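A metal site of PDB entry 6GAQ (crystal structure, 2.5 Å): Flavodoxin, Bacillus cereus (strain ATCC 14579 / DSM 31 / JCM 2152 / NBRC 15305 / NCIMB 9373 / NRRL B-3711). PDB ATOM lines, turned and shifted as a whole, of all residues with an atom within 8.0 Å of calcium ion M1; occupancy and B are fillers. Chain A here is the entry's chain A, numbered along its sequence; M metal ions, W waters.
N of Asp 139 sits close to OD1 of Asp 136 (3.5 Å). The side-chain carboxylate (OD2) of Asp 139 lies within salt-bridge range of the side-chain amino group (NZ) of Lys 142 (3.995 Å).
Three residues have an atom within 4 Å of calcium ion M1: Glu 131, Ala 133 and Asp 139.
Calcium ion M1 is bound by the side-chain carboxylate (OD1) of Asp 139 (2.4 Å), the backbone carbonyl oxygen (O) of Ala 133 (2.4 Å), water W1 (2.5 Å) and the backbone carbonyl oxygen (O) of Glu 131 (2.5 Å).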
ATOM      1  N   ASN A  21       0.395   6.446  11.323  1.00  0.00           N
ATOM      2  CA  ASN A  21       1.607   6.325  10.511  1.00  0.00           C
ATOM      3  C   ASN A  21       2.464   5.158  10.970  1.00  0.00           C
ATOM      4  O   ASN A  21       2.894   4.327  10.158  1.00  0.00           O
ATOM      5  CB  ASN A  21       2.394   7.632  10.550  1.00  0.00           C
ATOM      6  CG  ASN A  21       1.575   8.823  10.112  1.00  0.00           C
ATOM      7  OD1 ASN A  21       0.715   8.711   9.235  1.00  0.00           O
ATOM      8  ND2 ASN A  21       1.837   9.974  10.723  1.00  0.00           N
ATOM      9  N   ILE A  25       3.351   1.341   9.239  1.00  0.00           N
ATOM     10  CA  ILE A  25       4.675   0.739   9.147  1.00  0.00           C
ATOM     11  C   ILE A  25       4.650  -0.664   9.749  1.00  0.00           C
ATOM     12  O   ILE A  25       5.243  -1.601   9.207  1.00  0.00           O
ATOM     13  CB  ILE A  25       5.720   1.627   9.831  1.00  0.00           C
ATOM     14  CG1 ILE A  25       5.724   3.029   9.218  1.00  0.00           C
ATOM     15  CG2 ILE A  25       7.100   1.005   9.715  1.00  0.00           C
ATOM     16  CD1 ILE A  25       6.496   4.042  10.024  1.00  0.00           C
ATOM     17  N   SER A  97       8.026   6.482  13.162  1.00  0.00           N
ATOM     18  CA  SER A  97       7.626   7.516  12.205  1.00  0.00           C
ATOM     19  C   SER A  97       7.716   8.870  12.881  1.00  0.00           C
ATOM     20  O   SER A  97       7.095   9.086  13.934  1.00  0.00           O
ATOM     21  CB  SER A  97       6.207   7.253  11.688  1.00  0.00           C
ATOM     22  OG  SER A  97       5.768   8.317  10.857  1.00  0.00           O
ATOM     23  N   GLY A  98       8.468   9.798  12.279  1.00  0.00           N
ATOM     24  CA  GLY A  98       8.639  11.130  12.794  1.00  0.00           C
ATOM     25  C   GLY A  98       8.333  12.181  11.740  1.00  0.00           C
ATOM     26  O   GLY A  98       7.577  11.954  10.801  1.00  0.00           O
ATOM     27  N   ILE A 130      11.014   6.461   9.369  1.00  0.00           N
ATOM     28  CA  ILE A 130      10.107   6.878   8.310  1.00  0.00           C
ATOM     29  C   ILE A 130       9.567   8.255   8.672  1.00  0.00           C
ATOM     30  O   ILE A 130       9.326   8.532   9.851  1.00  0.00           O
ATOM     31  CB  ILE A 130       8.967   5.860   8.124  1.00  0.00           C
ATOM     32  CG1 ILE A 130       9.512   4.523   7.580  1.00  0.00           C
ATOM     33  CG2 ILE A 130       7.863   6.403   7.216  1.00  0.00           C
ATOM     34  CD1 ILE A 130       9.812   4.536   6.079  1.00  0.00           C
ATOM     35  N   GLU A 131       9.384   9.115   7.666  1.00  0.00           N
ATOM     36  CA  GLU A 131       8.809  10.434   7.909  1.00  0.00           C
ATOM     37  C   GLU A 131       7.322  10.389   7.608  1.00  0.00           C
ATOM     38  O   GLU A 131       6.908  10.092   6.478  1.00  0.00           O
ATOM     39  CB  GLU A 131       9.514  11.505   7.083  1.00  0.00           C
ATOM     40  CG  GLU A 131       8.713  12.803   6.944  1.00  0.00           C
ATOM     41  CD  GLU A 131       9.594  13.995   6.584  1.00  0.00           C
ATOM     42  OE1 GLU A 131       9.285  15.129   7.030  1.00  0.00           O
ATOM     43  OE2 GLU A 131      10.584  13.821   5.849  1.00  0.00           O
ATOM     44  N   LEU A 132       6.513  10.661   8.640  1.00  0.00           N
ATOM     45  CA  LEU A 132       5.050  10.717   8.533  1.00  0.00           C
ATOM     46  C   LEU A 132       4.567   9.328   8.107  1.00  0.00           C
ATOM     47  O   LEU A 132       5.085   8.333   8.643  1.00  0.00           O
ATOM     48  CB  LEU A 132       4.658  11.865   7.592  1.00  0.00           C
ATOM     49  CG  LEU A 132       4.931  13.279   8.119  1.00  0.00           C
ATOM     50  CD1 LEU A 132       4.398  14.322   7.146  1.00  0.00           C
ATOM     51  CD2 LEU A 132       4.320  13.447   9.496  1.00  0.00           C
ATOM     52  N   ALA A 133       3.619   9.214   7.161  1.00  0.00           N
ATOM     53  CA  ALA A 133       3.104   7.927   6.719  1.00  0.00           C
ATOM     54  C   ALA A 133       3.974   7.341   5.608  1.00  0.00           C
ATOM     55  O   ALA A 133       4.552   8.088   4.814  1.00  0.00           O
ATOM     56  CB  ALA A 133       1.676   8.085   6.206  1.00  0.00           C
ATOM     57  N   PRO A 134       4.093   6.013   5.551  1.00  0.00           N
ATOM     58  CA  PRO A 134       4.818   5.363   4.448  1.00  0.00           C
ATOM     59  C   PRO A 134       3.984   5.297   3.172  1.00  0.00           C
ATOM     60  O   PRO A 134       3.621   4.219   2.687  1.00  0.00           O
ATOM     61  CB  PRO A 134       5.128   3.986   5.023  1.00  0.00           C
ATOM     62  CG  PRO A 134       3.969   3.705   5.919  1.00  0.00           C
ATOM     63  CD  PRO A 134       3.577   5.029   6.525  1.00  0.00           C
ATOM     64  N   GLU A 135       3.665   6.468   2.623  1.00  0.00           N
ATOM     65  CA  GLU A 135       2.666   6.602   1.569  1.00  0.00           C
ATOM     66  C   GLU A 135       3.282   6.889   0.193  1.00  0.00           C
ATOM     67  O   GLU A 135       2.642   7.512  -0.657  1.00  0.00           O
ATOM     68  CB  GLU A 135       1.660   7.693   1.931  1.00  0.00           C
ATOM     69  CG  GLU A 135       2.252   9.074   2.064  1.00  0.00           C
ATOM     70  CD  GLU A 135       1.301  10.068   2.716  1.00  0.00           C
ATOM     71  OE1 GLU A 135       1.559  10.473   3.867  1.00  0.00           O
ATOM     72  OE2 GLU A 135       0.301  10.428   2.070  1.00  0.00           O
ATOM     73  N   ASP A 136       4.522   6.456  -0.042  1.00  0.00           N
ATOM     74  CA  ASP A 136       5.137   6.599  -1.351  1.00  0.00           C
ATOM     75  C   ASP A 136       6.051   5.403  -1.588  1.00  0.00           C
ATOM     76  O   ASP A 136       6.252   4.559  -0.708  1.00  0.00           O
ATOM     77  CB  ASP A 136       5.874   7.931  -1.487  1.00  0.00           C
ATOM     78  CG  ASP A 136       7.172   7.956  -0.721  1.00  0.00           C
ATOM     79  OD1 ASP A 136       7.160   7.655   0.491  1.00  0.00           O
ATOM     80  OD2 ASP A 136       8.212   8.288  -1.328  1.00  0.00           O
ATOM     81  N   GLU A 138       9.374   4.872  -2.143  1.00  0.00           N
ATOM     82  CA  GLU A 138      10.615   4.632  -1.428  1.00  0.00           C
ATOM     83  C   GLU A 138      10.425   4.475   0.070  1.00  0.00           C
ATOM     84  O   GLU A 138      11.313   3.949   0.740  1.00  0.00           O
ATOM     85  CB  GLU A 138      11.638   5.741  -1.716  1.00  0.00           C
ATOM     86  CG  GLU A 138      11.073   7.142  -1.768  1.00  0.00           C
ATOM     87  CD  GLU A 138      12.019   8.125  -2.424  1.00  0.00           C
ATOM     88  OE1 GLU A 138      11.883   9.345  -2.197  1.00  0.00           O
ATOM     89  OE2 GLU A 138      12.916   7.668  -3.176  1.00  0.00           O
ATOM     90  N   ASP A 139       9.281   4.909   0.621  1.00  0.00           N
ATOM     91  CA  ASP A 139       8.978   4.580   2.008  1.00  0.00           C
ATOM     92  C   ASP A 139       8.570   3.110   2.133  1.00  0.00           C
ATOM     93  O   ASP A 139       8.986   2.430   3.074  1.00  0.00           O
ATOM     94  CB  ASP A 139       7.867   5.478   2.545  1.00  0.00           C
ATOM     95  CG  ASP A 139       8.400   6.676   3.295  1.00  0.00           C
ATOM     96  OD1 ASP A 139       7.618   7.297   4.045  1.00  0.00           O
ATOM     97  OD2 ASP A 139       9.599   6.997   3.146  1.00  0.00           O
ATOM     98  N   VAL A 140       7.760   2.625   1.198  1.00  0.00           N
ATOM     99  CA  VAL A 140       7.390   1.210   1.188  1.00  0.00           C
ATOM    100  C   VAL A 140       8.627   0.344   0.980  1.00  0.00           C
ATOM    101  O   VAL A 140       8.753  -0.736   1.584  1.00  0.00           O
ATOM    102  CB  VAL A 140       6.330   0.952   0.101  1.00  0.00           C
ATOM    103  CG1 VAL A 140       5.993  -0.528   0.021  1.00  0.00           C
ATOM    104  CG2 VAL A 140       5.073   1.772   0.375  1.00  0.00           C
ATOM    105  N   LYS A 142      11.653   1.236   1.886  1.00  0.00           N
ATOM    106  CA  LYS A 142      12.407   1.324   3.129  1.00  0.00           C
ATOM    107  C   LYS A 142      11.937   0.283   4.127  1.00  0.00           C
ATOM    108  O   LYS A 142      12.746  -0.415   4.760  1.00  0.00           O
ATOM    109  CB  LYS A 142      12.303   2.726   3.722  1.00  0.00           C
ATOM    110  CG  LYS A 142      13.322   3.719   3.188  1.00  0.00           C
ATOM    111  CD  LYS A 142      12.936   5.155   3.528  1.00  0.00           C
ATOM    112  CE  LYS A 142      13.280   5.497   4.968  1.00  0.00           C
ATOM    113  NZ  LYS A 142      12.974   6.918   5.283  1.00  0.00           N
HETATM  114 CA    CA M   1       6.503   9.387   4.143  1.00  0.00          CA
HETATM  115 CA    CA M   2      10.083  10.027  -0.651  1.00  0.00          CA
HETATM  116  O   HOH W   1       4.955  11.300   4.052  1.00  0.00           O
